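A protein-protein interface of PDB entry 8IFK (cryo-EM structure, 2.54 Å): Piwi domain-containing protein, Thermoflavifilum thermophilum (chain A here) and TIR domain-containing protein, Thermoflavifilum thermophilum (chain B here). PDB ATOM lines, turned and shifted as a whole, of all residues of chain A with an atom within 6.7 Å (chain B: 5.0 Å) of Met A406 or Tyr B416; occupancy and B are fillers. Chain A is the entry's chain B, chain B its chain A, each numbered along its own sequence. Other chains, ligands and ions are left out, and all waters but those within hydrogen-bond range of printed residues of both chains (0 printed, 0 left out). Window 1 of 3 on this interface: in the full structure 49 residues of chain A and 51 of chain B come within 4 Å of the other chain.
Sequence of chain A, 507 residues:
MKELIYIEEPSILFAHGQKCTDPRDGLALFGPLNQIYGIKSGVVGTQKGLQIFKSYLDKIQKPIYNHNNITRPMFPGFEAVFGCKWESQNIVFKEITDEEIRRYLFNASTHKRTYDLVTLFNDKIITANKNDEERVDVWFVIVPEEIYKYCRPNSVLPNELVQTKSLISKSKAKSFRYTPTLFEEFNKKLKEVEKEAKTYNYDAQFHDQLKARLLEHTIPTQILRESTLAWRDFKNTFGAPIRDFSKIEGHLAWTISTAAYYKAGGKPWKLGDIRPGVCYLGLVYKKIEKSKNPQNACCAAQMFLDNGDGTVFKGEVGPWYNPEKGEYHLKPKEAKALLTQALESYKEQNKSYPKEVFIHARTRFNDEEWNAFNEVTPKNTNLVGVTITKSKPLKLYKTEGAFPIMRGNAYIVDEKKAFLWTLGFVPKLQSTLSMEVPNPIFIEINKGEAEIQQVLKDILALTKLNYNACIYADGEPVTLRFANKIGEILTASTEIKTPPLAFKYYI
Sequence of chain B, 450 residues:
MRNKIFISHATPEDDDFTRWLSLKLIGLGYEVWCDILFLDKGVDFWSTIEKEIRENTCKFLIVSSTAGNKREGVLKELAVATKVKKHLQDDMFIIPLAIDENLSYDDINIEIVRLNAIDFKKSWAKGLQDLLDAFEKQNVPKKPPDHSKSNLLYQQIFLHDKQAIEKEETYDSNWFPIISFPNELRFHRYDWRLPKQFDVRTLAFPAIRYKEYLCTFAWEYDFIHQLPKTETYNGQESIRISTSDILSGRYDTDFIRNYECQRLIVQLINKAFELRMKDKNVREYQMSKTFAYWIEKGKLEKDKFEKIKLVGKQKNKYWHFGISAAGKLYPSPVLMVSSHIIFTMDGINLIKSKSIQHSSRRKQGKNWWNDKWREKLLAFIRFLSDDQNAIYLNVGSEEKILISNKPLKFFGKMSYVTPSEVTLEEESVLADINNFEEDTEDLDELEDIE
The side-chain hydroxyl of Tyr B416 sits at hydrogen-bond distance from the side-chain amino group of Lys A398, 3.1 Å away.
The side-chain hydroxyl (OH) of Tyr B416 lies close to the backbone carbonyl oxygen (O) of Pro A404, at 2.2 Å.
The side-chain amide nitrogen of Asn A409 sits at hydrogen-bond distance from the side-chain hydroxyl of Tyr B171 (3.4 Å).
The side-chain amino group (NZ) of Lys A398 is in hydrogen-bond range of the side-chain hydroxyl (OG1) of Thr B418 (3.3 Å).
OH of Tyr B416 lies close to O of Phe A403 (3.1 Å).
The backbone carbonyl oxygen of Asn A409 lies within hydrogen-bond range of the backbone NH of Trp A421 (3.0 Å).
The backbone NH (N) of Arg A407 is in hydrogen-bond range of the backbone carbonyl oxygen (O) of Phe A425 (2.7 Å).
The backbone carbonyl oxygen of Tyr B416 sits at hydrogen-bond distance from the side-chain amino group of Lys B167.
O of Met A406 is in hydrogen-bond range of ND2 of Asn A409 (3.0 Å).
The backbone carbonyl oxygen (O) of Pro A427 is in hydrogen-bond range of the side-chain amide nitrogen (NE2) of Gln A430.
N of Ile B165 is in hydrogen-bond range of O of Ser B415 (2.8 Å).
Of chain B, only Ala B164 (3.6 Å), Met B414 (3.5 Å), Ser B415 (3.6 Å) and Tyr B416 (3.5 Å) come within 4 Å of Met A406.
Printed residues of chain B within 4 Å of Asn A409: Tyr B171.
Of the printed residues of chain B, Pro A404 touches Tyr B416.
Of the printed residues of chain B, Phe A425 touches Tyr B416 and Pro B419.
Printed residues of chain A within 4 Å of Thr B418: Lys A398 (3.3 Å) and Phe A403 (3.5 Å).
Of the printed residues of chain B, Ile A405 touches Tyr B171.
Val B417 touches none of the printed residues of chain A.
The nearest residue of chain B that does not touch Met A406 is Tyr B171 (4.6 Å).
Among the printed residues, pairs that only touch across the chains: Tyr A6 with Ala B164 (3.4 Å), Tyr A6 with Met B414 (3.5 Å), Lys A398 with Tyr B171 (3.7 Å), Phe A403 with Thr B418 (3.5 Å), Phe A403 with Pro B419 (3.7 Å), Ile A405 with Tyr B171 (3.6 Å), Met A406 with Ala B164 (3.6 Å), Met A406 with Met B414 (3.5 Å), Met A406 with Ser B415 (3.6 Å), Met A406 with Tyr B416 (3.5 Å), Phe A425 with Tyr B416 (3.3 Å), Phe A425 with Pro B419 (3.5 Å), Pro A427 with Gln B163 (3.4 Å), Pro A427 with Ala B164 (3.9 Å) and Gln A430 with Pro B419 (3.6 Å).
Of the 11 printed residues of chain B, 8 touch a printed residue of chain A.
Printed residues of chain B that touch a printed residue of chain A: Gln B163, Ala B164, Tyr B171, Met B414, Ser B415, Tyr B416, Thr B418 and Pro B419.
Hydrophobic or aromatic side chains of chain B within 4 Å of the printed part of chain A: Ala B164, Tyr B171, Met B414, Tyr B416 and Pro B419.
Of the 21 printed residues of chain A, 10 touch a printed residue of chain B.
Printed residues of chain A that touch a printed residue of chain B: Tyr A6, Lys A398, Phe A403, Pro A404, Ile A405, Met A406, Asn A409, Phe A425, Pro A427 and Gln A430.
Hydrophobic or aromatic side chains of chain A that line the printed part of chain B: Tyr A6, Phe A403, Ile A405, Met A406, Phe A425 and Pro A427.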
ATOM      1  N   TYR A   6       6.213 -32.113  -9.350  1.00  0.00           N
ATOM      2  CA  TYR A   6       5.238 -31.370 -10.133  1.00  0.00           C
ATOM      3  C   TYR A   6       3.888 -31.432  -9.440  1.00  0.00           C
ATOM      4  O   TYR A   6       3.393 -32.521  -9.129  1.00  0.00           O
ATOM      5  CB  TYR A   6       5.129 -31.925 -11.553  1.00  0.00           C
ATOM      6  CG  TYR A   6       4.044 -31.274 -12.380  1.00  0.00           C
ATOM      7  CD1 TYR A   6       4.176 -29.969 -12.831  1.00  0.00           C
ATOM      8  CD2 TYR A   6       2.884 -31.965 -12.705  1.00  0.00           C
ATOM      9  CE1 TYR A   6       3.186 -29.371 -13.582  1.00  0.00           C
ATOM     10  CE2 TYR A   6       1.890 -31.376 -13.458  1.00  0.00           C
ATOM     11  CZ  TYR A   6       2.045 -30.079 -13.894  1.00  0.00           C
ATOM     12  OH  TYR A   6       1.056 -29.487 -14.644  1.00  0.00           O
ATOM     13  N   LYS A 398      15.124 -23.429 -17.799  1.00  0.00           N
ATOM     14  CA  LYS A 398      15.015 -24.608 -18.649  1.00  0.00           C
ATOM     15  C   LYS A 398      16.188 -24.644 -19.619  1.00  0.00           C
ATOM     16  O   LYS A 398      16.296 -23.788 -20.502  1.00  0.00           O
ATOM     17  CB  LYS A 398      13.683 -24.608 -19.402  1.00  0.00           C
ATOM     18  CG  LYS A 398      13.007 -25.965 -19.464  1.00  0.00           C
ATOM     19  CD  LYS A 398      11.816 -25.959 -20.408  1.00  0.00           C
ATOM     20  CE  LYS A 398      12.232 -25.588 -21.823  1.00  0.00           C
ATOM     21  NZ  LYS A 398      11.095 -25.672 -22.778  1.00  0.00           N
ATOM     22  N   GLY A 401      15.297 -25.432 -23.845  1.00  0.00           N
ATOM     23  CA  GLY A 401      14.469 -24.575 -24.658  1.00  0.00           C
ATOM     24  C   GLY A 401      14.542 -23.099 -24.294  1.00  0.00           C
ATOM     25  O   GLY A 401      15.194 -22.681 -23.341  1.00  0.00           O
ATOM     26  N   ALA A 402      13.838 -22.309 -25.102  1.00  0.00           N
ATOM     27  CA  ALA A 402      13.720 -20.873 -24.900  1.00  0.00           C
ATOM     28  C   ALA A 402      12.574 -20.493 -23.974  1.00  0.00           C
ATOM     29  O   ALA A 402      12.455 -19.320 -23.609  1.00  0.00           O
ATOM     30  CB  ALA A 402      13.539 -20.163 -26.245  1.00  0.00           C
ATOM     31  N   PHE A 403      11.740 -21.445 -23.594  1.00  0.00           N
ATOM     32  CA  PHE A 403      10.611 -21.216 -22.712  1.00  0.00           C
ATOM     33  C   PHE A 403      10.952 -21.655 -21.296  1.00  0.00           C
ATOM     34  O   PHE A 403      11.789 -22.537 -21.091  1.00  0.00           O
ATOM     35  CB  PHE A 403       9.380 -21.967 -23.230  1.00  0.00           C
ATOM     36  CG  PHE A 403       8.719 -21.299 -24.403  1.00  0.00           C
ATOM     37  CD1 PHE A 403       9.284 -21.367 -25.664  1.00  0.00           C
ATOM     38  CD2 PHE A 403       7.544 -20.589 -24.239  1.00  0.00           C
ATOM     39  CE1 PHE A 403       8.684 -20.751 -26.742  1.00  0.00           C
ATOM     40  CE2 PHE A 403       6.938 -19.972 -25.314  1.00  0.00           C
ATOM     41  CZ  PHE A 403       7.509 -20.052 -26.567  1.00  0.00           C
ATOM     42  N   PRO A 404      10.327 -21.050 -20.282  1.00  0.00           N
ATOM     43  CA  PRO A 404      10.805 -21.248 -18.909  1.00  0.00           C
ATOM     44  C   PRO A 404      10.289 -22.513 -18.249  1.00  0.00           C
ATOM     45  O   PRO A 404       9.639 -23.349 -18.883  1.00  0.00           O
ATOM     46  CB  PRO A 404      10.286 -20.001 -18.188  1.00  0.00           C
ATOM     47  CG  PRO A 404       9.018 -19.695 -18.889  1.00  0.00           C
ATOM     48  CD  PRO A 404       9.180 -20.125 -20.326  1.00  0.00           C
ATOM     49  N   ILE A 405      10.600 -22.654 -16.960  1.00  0.00           N
ATOM     50  CA  ILE A 405      10.118 -23.789 -16.187  1.00  0.00           C
ATOM     51  C   ILE A 405       8.598 -23.755 -16.118  1.00  0.00           C
ATOM     52  O   ILE A 405       7.985 -22.702 -15.903  1.00  0.00           O
ATOM     53  CB  ILE A 405      10.752 -23.770 -14.786  1.00  0.00           C
ATOM     54  CG1 ILE A 405      10.104 -24.809 -13.872  1.00  0.00           C
ATOM     55  CG2 ILE A 405      10.668 -22.380 -14.181  1.00  0.00           C
ATOM     56  CD1 ILE A 405      10.960 -25.176 -12.690  1.00  0.00           C
ATOM     57  N   MET A 406       7.981 -24.917 -16.317  1.00  0.00           N
ATOM     58  CA  MET A 406       6.530 -25.009 -16.337  1.00  0.00           C
ATOM     59  C   MET A 406       5.951 -24.701 -14.962  1.00  0.00           C
ATOM     60  O   MET A 406       6.508 -25.095 -13.933  1.00  0.00           O
ATOM     61  CB  MET A 406       6.104 -26.405 -16.792  1.00  0.00           C
ATOM     62  CG  MET A 406       4.663 -26.764 -16.487  1.00  0.00           C
ATOM     63  SD  MET A 406       4.251 -28.423 -17.043  1.00  0.00           S
ATOM     64  CE  MET A 406       5.526 -29.366 -16.217  1.00  0.00           C
ATOM     65  N   ARG A 407       4.830 -23.981 -14.947  1.00  0.00           N
ATOM     66  CA  ARG A 407       4.141 -23.705 -13.694  1.00  0.00           C
ATOM     67  C   ARG A 407       3.679 -25.006 -13.047  1.00  0.00           C
ATOM     68  O   ARG A 407       3.217 -25.927 -13.725  1.00  0.00           O
ATOM     69  CB  ARG A 407       2.946 -22.781 -13.931  1.00  0.00           C
ATOM     70  CG  ARG A 407       1.856 -22.930 -12.884  1.00  0.00           C
ATOM     71  CD  ARG A 407       0.693 -21.989 -13.096  1.00  0.00           C
ATOM     72  NE  ARG A 407      -0.463 -22.422 -12.321  1.00  0.00           N
ATOM     73  CZ  ARG A 407      -0.812 -21.911 -11.149  1.00  0.00           C
ATOM     74  NH1 ARG A 407      -0.119 -20.935 -10.586  1.00  0.00           N
ATOM     75  NH2 ARG A 407      -1.887 -22.388 -10.528  1.00  0.00           N
ATOM     76  N   GLY A 408       3.802 -25.074 -11.724  1.00  0.00           N
ATOM     77  CA  GLY A 408       3.466 -26.261 -10.972  1.00  0.00           C
ATOM     78  C   GLY A 408       4.657 -27.082 -10.534  1.00  0.00           C
ATOM     79  O   GLY A 408       4.509 -27.932  -9.648  1.00  0.00           O
ATOM     80  N   ASN A 409       5.824 -26.858 -11.128  1.00  0.00           N
ATOM     81  CA  ASN A 409       7.039 -27.496 -10.647  1.00  0.00           C
ATOM     82  C   ASN A 409       7.404 -26.935  -9.280  1.00  0.00           C
ATOM     83  O   ASN A 409       7.289 -25.732  -9.035  1.00  0.00           O
ATOM     84  CB  ASN A 409       8.185 -27.271 -11.632  1.00  0.00           C
ATOM     85  CG  ASN A 409       8.157 -28.247 -12.789  1.00  0.00           C
ATOM     86  OD1 ASN A 409       8.321 -29.453 -12.605  1.00  0.00           O
ATOM     87  ND2 ASN A 409       7.950 -27.729 -13.993  1.00  0.00           N
ATOM     88  N   ALA A 410       7.830 -27.814  -8.380  1.00  0.00           N
ATOM     89  CA  ALA A 410       8.137 -27.422  -7.013  1.00  0.00           C
ATOM     90  C   ALA A 410       9.441 -28.064  -6.567  1.00  0.00           C
ATOM     91  O   ALA A 410       9.641 -29.268  -6.754  1.00  0.00           O
ATOM     92  CB  ALA A 410       7.004 -27.811  -6.062  1.00  0.00           C
ATOM     93  N   TRP A 421       6.548 -22.999  -8.145  1.00  0.00           N
ATOM     94  CA  TRP A 421       6.448 -22.192  -9.356  1.00  0.00           C
ATOM     95  C   TRP A 421       4.972 -22.022  -9.696  1.00  0.00           C
ATOM     96  O   TRP A 421       4.416 -22.698 -10.561  1.00  0.00           O
ATOM     97  CB  TRP A 421       7.232 -22.828 -10.499  1.00  0.00           C
ATOM     98  CG  TRP A 421       8.653 -22.371 -10.548  1.00  0.00           C
ATOM     99  CD1 TRP A 421       9.156 -21.344 -11.288  1.00  0.00           C
ATOM    100  CD2 TRP A 421       9.754 -22.914  -9.812  1.00  0.00           C
ATOM    101  NE1 TRP A 421      10.505 -21.218 -11.066  1.00  0.00           N
ATOM    102  CE2 TRP A 421      10.896 -22.171 -10.164  1.00  0.00           C
ATOM    103  CE3 TRP A 421       9.886 -23.959  -8.894  1.00  0.00           C
ATOM    104  CZ2 TRP A 421      12.152 -22.438  -9.629  1.00  0.00           C
ATOM    105  CZ3 TRP A 421      11.132 -24.222  -8.365  1.00  0.00           C
ATOM    106  CH2 TRP A 421      12.248 -23.465  -8.731  1.00  0.00           C
ATOM    107  N   LEU A 423       4.109 -19.448 -11.106  1.00  0.00           N
ATOM    108  CA  LEU A 423       4.272 -18.836 -12.410  1.00  0.00           C
ATOM    109  C   LEU A 423       5.224 -19.686 -13.237  1.00  0.00           C
ATOM    110  O   LEU A 423       5.853 -20.624 -12.741  1.00  0.00           O
ATOM    111  CB  LEU A 423       4.801 -17.404 -12.286  1.00  0.00           C
ATOM    112  CG  LEU A 423       3.998 -16.522 -11.336  1.00  0.00           C
ATOM    113  CD1 LEU A 423       4.931 -15.677 -10.493  1.00  0.00           C
ATOM    114  CD2 LEU A 423       3.023 -15.663 -12.118  1.00  0.00           C
ATOM    115  N   GLY A 424       5.328 -19.345 -14.510  1.00  0.00           N
ATOM    116  CA  GLY A 424       6.112 -20.102 -15.452  1.00  0.00           C
ATOM    117  C   GLY A 424       5.268 -20.497 -16.632  1.00  0.00           C
ATOM    118  O   GLY A 424       4.163 -19.984 -16.839  1.00  0.00           O
ATOM    119  N   PHE A 425       5.789 -21.421 -17.430  1.00  0.00           N
ATOM    120  CA  PHE A 425       5.063 -21.862 -18.609  1.00  0.00           C
ATOM    121  C   PHE A 425       3.795 -22.600 -18.205  1.00  0.00           C
ATOM    122  O   PHE A 425       3.825 -23.496 -17.356  1.00  0.00           O
ATOM    123  CB  PHE A 425       5.936 -22.761 -19.478  1.00  0.00           C
ATOM    124  CG  PHE A 425       5.339 -23.057 -20.820  1.00  0.00           C
ATOM    125  CD1 PHE A 425       5.544 -22.202 -21.887  1.00  0.00           C
ATOM    126  CD2 PHE A 425       4.554 -24.179 -21.010  1.00  0.00           C
ATOM    127  CE1 PHE A 425       4.988 -22.470 -23.118  1.00  0.00           C
ATOM    128  CE2 PHE A 425       3.995 -24.448 -22.239  1.00  0.00           C
ATOM    129  CZ  PHE A 425       4.216 -23.596 -23.293  1.00  0.00           C
ATOM    130  N   VAL A 426       2.680 -22.215 -18.813  1.00  0.00           N
ATOM    131  CA  VAL A 426       1.405 -22.902 -18.660  1.00  0.00           C
ATOM    132  C   VAL A 426       1.160 -23.692 -19.943  1.00  0.00           C
ATOM    133  O   VAL A 426       0.988 -23.091 -21.014  1.00  0.00           O
ATOM    134  CB  VAL A 426       0.260 -21.920 -18.381  1.00  0.00           C
ATOM    135  CG1 VAL A 426      -1.078 -22.610 -18.560  1.00  0.00           C
ATOM    136  CG2 VAL A 426       0.389 -21.350 -16.983  1.00  0.00           C
ATOM    137  N   PRO A 427       1.169 -25.027 -19.896  1.00  0.00           N
ATOM    138  CA  PRO A 427       0.950 -25.796 -21.132  1.00  0.00           C
ATOM    139  C   PRO A 427      -0.374 -25.486 -21.804  1.00  0.00           C
ATOM    140  O   PRO A 427      -0.433 -25.419 -23.037  1.00  0.00           O
ATOM    141  CB  PRO A 427       1.023 -27.250 -20.647  1.00  0.00           C
ATOM    142  CG  PRO A 427       1.842 -27.187 -19.402  1.00  0.00           C
ATOM    143  CD  PRO A 427       1.443 -25.902 -18.746  1.00  0.00           C
ATOM    144  N   GLN A 430       0.002 -22.323 -23.499  1.00  0.00           N
ATOM    145  CA  GLN A 430       1.126 -22.386 -24.432  1.00  0.00           C
ATOM    146  C   GLN A 430       2.025 -21.160 -24.313  1.00  0.00           C
ATOM    147  O   GLN A 430       2.611 -20.706 -25.300  1.00  0.00           O
ATOM    148  CB  GLN A 430       0.645 -22.566 -25.876  1.00  0.00           C
ATOM    149  CG  GLN A 430       0.250 -23.991 -26.217  1.00  0.00           C
ATOM    150  CD  GLN A 430       1.434 -24.934 -26.225  1.00  0.00           C
ATOM    151  OE1 GLN A 430       2.239 -24.929 -27.155  1.00  0.00           O
ATOM    152  NE2 GLN A 430       1.549 -25.749 -25.183  1.00  0.00           N
ATOM    153  N   THR A 432       3.823 -18.259 -20.935  1.00  0.00           N
ATOM    154  CA  THR A 432       4.219 -18.047 -19.553  1.00  0.00           C
ATOM    155  C   THR A 432       3.289 -17.054 -18.867  1.00  0.00           C
ATOM    156  O   THR A 432       2.854 -16.065 -19.463  1.00  0.00           O
ATOM    157  CB  THR A 432       5.660 -17.538 -19.485  1.00  0.00           C
ATOM    158  OG1 THR A 432       6.479 -18.305 -20.373  1.00  0.00           O
ATOM    159  CG2 THR A 432       6.210 -17.651 -18.078  1.00  0.00           C
ATOM    160  N   PRO A 438      10.322 -16.852 -14.526  1.00  0.00           N
ATOM    161  CA  PRO A 438       9.489 -16.730 -13.336  1.00  0.00           C
ATOM    162  C   PRO A 438      10.186 -16.745 -11.973  1.00  0.00           C
ATOM    163  O   PRO A 438      11.152 -17.416 -11.763  1.00  0.00           O
ATOM    164  CB  PRO A 438       8.688 -18.027 -13.348  1.00  0.00           C
ATOM    165  CG  PRO A 438       9.501 -18.964 -14.167  1.00  0.00           C
ATOM    166  CD  PRO A 438      10.085 -18.090 -15.239  1.00  0.00           C
ATOM    167  N   GLN B 163      -1.025 -29.906 -22.721  1.00  0.00           N
ATOM    168  CA  GLN B 163      -1.031 -30.538 -21.412  1.00  0.00           C
ATOM    169  C   GLN B 163       0.398 -30.674 -20.905  1.00  0.00           C
ATOM    170  O   GLN B 163       1.365 -30.458 -21.640  1.00  0.00           O
ATOM    171  CB  GLN B 163      -1.703 -31.924 -21.456  1.00  0.00           C
ATOM    172  CG  GLN B 163      -3.213 -31.965 -21.776  1.00  0.00           C
ATOM    173  CD  GLN B 163      -4.111 -31.093 -20.891  1.00  0.00           C
ATOM    174  OE1 GLN B 163      -3.648 -30.286 -20.085  1.00  0.00           O
ATOM    175  NE2 GLN B 163      -5.418 -31.258 -21.059  1.00  0.00           N
ATOM    176  N   ALA B 164       0.520 -31.032 -19.629  1.00  0.00           N
ATOM    177  CA  ALA B 164       1.809 -31.348 -19.026  1.00  0.00           C
ATOM    178  C   ALA B 164       2.086 -32.832 -19.222  1.00  0.00           C
ATOM    179  O   ALA B 164       1.331 -33.679 -18.734  1.00  0.00           O
ATOM    180  CB  ALA B 164       1.818 -30.986 -17.542  1.00  0.00           C
ATOM    181  N   ILE B 165       3.165 -33.145 -19.932  1.00  0.00           N
ATOM    182  CA  ILE B 165       3.459 -34.511 -20.328  1.00  0.00           C
ATOM    183  C   ILE B 165       4.545 -35.081 -19.427  1.00  0.00           C
ATOM    184  O   ILE B 165       5.231 -34.364 -18.693  1.00  0.00           O
ATOM    185  CB  ILE B 165       3.873 -34.594 -21.814  1.00  0.00           C
ATOM    186  CG1 ILE B 165       5.307 -34.100 -21.995  1.00  0.00           C
ATOM    187  CG2 ILE B 165       2.915 -33.790 -22.678  1.00  0.00           C
ATOM    188  CD1 ILE B 165       5.734 -33.972 -23.437  1.00  0.00           C
ATOM    189  N   LYS B 167       7.612 -35.798 -19.389  1.00  0.00           N
ATOM    190  CA  LYS B 167       8.874 -35.479 -20.042  1.00  0.00           C
ATOM    191  C   LYS B 167       9.928 -35.180 -18.987  1.00  0.00           C
ATOM    192  O   LYS B 167       9.695 -34.371 -18.082  1.00  0.00           O
ATOM    193  CB  LYS B 167       8.709 -34.286 -20.984  1.00  0.00           C
ATOM    194  CG  LYS B 167       9.975 -33.857 -21.703  1.00  0.00           C
ATOM    195  CD  LYS B 167       9.640 -33.016 -22.925  1.00  0.00           C
ATOM    196  CE  LYS B 167      10.385 -31.692 -22.901  1.00  0.00           C
ATOM    197  NZ  LYS B 167      10.458 -31.064 -24.248  1.00  0.00           N
ATOM    198  N   TYR B 171      16.937 -28.369 -15.561  1.00  0.00           N
ATOM    199  CA  TYR B 171      16.943 -26.935 -15.324  1.00  0.00           C
ATOM    200  C   TYR B 171      18.263 -26.497 -14.706  1.00  0.00           C
ATOM    201  O   TYR B 171      18.807 -27.177 -13.829  1.00  0.00           O
ATOM    202  CB  TYR B 171      15.794 -26.511 -14.396  1.00  0.00           C
ATOM    203  CG  TYR B 171      14.437 -27.056 -14.777  1.00  0.00           C
ATOM    204  CD1 TYR B 171      14.024 -28.309 -14.344  1.00  0.00           C
ATOM    205  CD2 TYR B 171      13.564 -26.313 -15.557  1.00  0.00           C
ATOM    206  CE1 TYR B 171      12.784 -28.808 -14.687  1.00  0.00           C
ATOM    207  CE2 TYR B 171      12.324 -26.805 -15.904  1.00  0.00           C
ATOM    208  CZ  TYR B 171      11.938 -28.052 -15.464  1.00  0.00           C
ATOM    209  OH  TYR B 171      10.701 -28.545 -15.807  1.00  0.00           O
ATOM    210  N   MET B 414       8.117 -33.971 -15.204  1.00  0.00           N
ATOM    211  CA  MET B 414       7.028 -33.370 -15.958  1.00  0.00           C
ATOM    212  C   MET B 414       7.560 -32.180 -16.742  1.00  0.00           C
ATOM    213  O   MET B 414       8.381 -31.411 -16.234  1.00  0.00           O
ATOM    214  CB  MET B 414       5.898 -32.913 -15.033  1.00  0.00           C
ATOM    215  CG  MET B 414       5.066 -34.035 -14.433  1.00  0.00           C
ATOM    216  SD  MET B 414       3.857 -34.750 -15.559  1.00  0.00           S
ATOM    217  CE  MET B 414       4.306 -36.479 -15.455  1.00  0.00           C
ATOM    218  N   SER B 415       7.090 -32.031 -17.975  1.00  0.00           N
ATOM    219  CA  SER B 415       7.469 -30.899 -18.810  1.00  0.00           C
ATOM    220  C   SER B 415       6.387 -30.701 -19.863  1.00  0.00           C
ATOM    221  O   SER B 415       5.295 -31.269 -19.779  1.00  0.00           O
ATOM    222  CB  SER B 415       8.844 -31.109 -19.446  1.00  0.00           C
ATOM    223  OG  SER B 415       9.430 -29.870 -19.807  1.00  0.00           O
ATOM    224  N   TYR B 416       6.700 -29.880 -20.859  1.00  0.00           N
ATOM    225  CA  TYR B 416       5.771 -29.546 -21.923  1.00  0.00           C
ATOM    226  C   TYR B 416       6.475 -29.614 -23.270  1.00  0.00           C
ATOM    227  O   TYR B 416       7.701 -29.516 -23.361  1.00  0.00           O
ATOM    228  CB  TYR B 416       5.184 -28.141 -21.733  1.00  0.00           C
ATOM    229  CG  TYR B 416       6.229 -27.073 -21.506  1.00  0.00           C
ATOM    230  CD1 TYR B 416       6.737 -26.827 -20.239  1.00  0.00           C
ATOM    231  CD2 TYR B 416       6.723 -26.323 -22.566  1.00  0.00           C
ATOM    232  CE1 TYR B 416       7.693 -25.856 -20.030  1.00  0.00           C
ATOM    233  CE2 TYR B 416       7.678 -25.349 -22.365  1.00  0.00           C
ATOM    234  CZ  TYR B 416       8.159 -25.121 -21.096  1.00  0.00           C
ATOM    235  OH  TYR B 416       9.112 -24.154 -20.891  1.00  0.00           O
ATOM    236  N   VAL B 417       5.678 -29.785 -24.323  1.00  0.00           N
ATOM    237  CA  VAL B 417       6.197 -29.634 -25.675  1.00  0.00           C
ATOM    238  C   VAL B 417       6.369 -28.150 -25.966  1.00  0.00           C
ATOM    239  O   VAL B 417       5.417 -27.366 -25.860  1.00  0.00           O
ATOM    240  CB  VAL B 417       5.263 -30.305 -26.692  1.00  0.00           C
ATOM    241  CG1 VAL B 417       5.810 -30.143 -28.100  1.00  0.00           C
ATOM    242  CG2 VAL B 417       5.080 -31.775 -26.353  1.00  0.00           C
ATOM    243  N   THR B 418       7.587 -27.760 -26.326  1.00  0.00           N
ATOM    244  CA  THR B 418       7.893 -26.349 -26.507  1.00  0.00           C
ATOM    245  C   THR B 418       7.096 -25.776 -27.677  1.00  0.00           C
ATOM    246  O   THR B 418       6.996 -26.413 -28.732  1.00  0.00           O
ATOM    247  CB  THR B 418       9.391 -26.160 -26.751  1.00  0.00           C
ATOM    248  OG1 THR B 418      10.131 -26.848 -25.736  1.00  0.00           O
ATOM    249  CG2 THR B 418       9.760 -24.687 -26.723  1.00  0.00           C
ATOM    250  N   PRO B 419       6.500 -24.594 -27.516  1.00  0.00           N
ATOM    251  CA  PRO B 419       5.808 -23.962 -28.644  1.00  0.00           C
ATOM    252  C   PRO B 419       6.758 -23.704 -29.803  1.00  0.00           C
ATOM    253  O   PRO B 419       7.930 -23.374 -29.610  1.00  0.00           O
ATOM    254  CB  PRO B 419       5.280 -22.652 -28.048  1.00  0.00           C
ATOM    255  CG  PRO B 419       5.168 -22.920 -26.595  1.00  0.00           C
ATOM    256  CD  PRO B 419       6.282 -23.868 -26.254  1.00  0.00           C
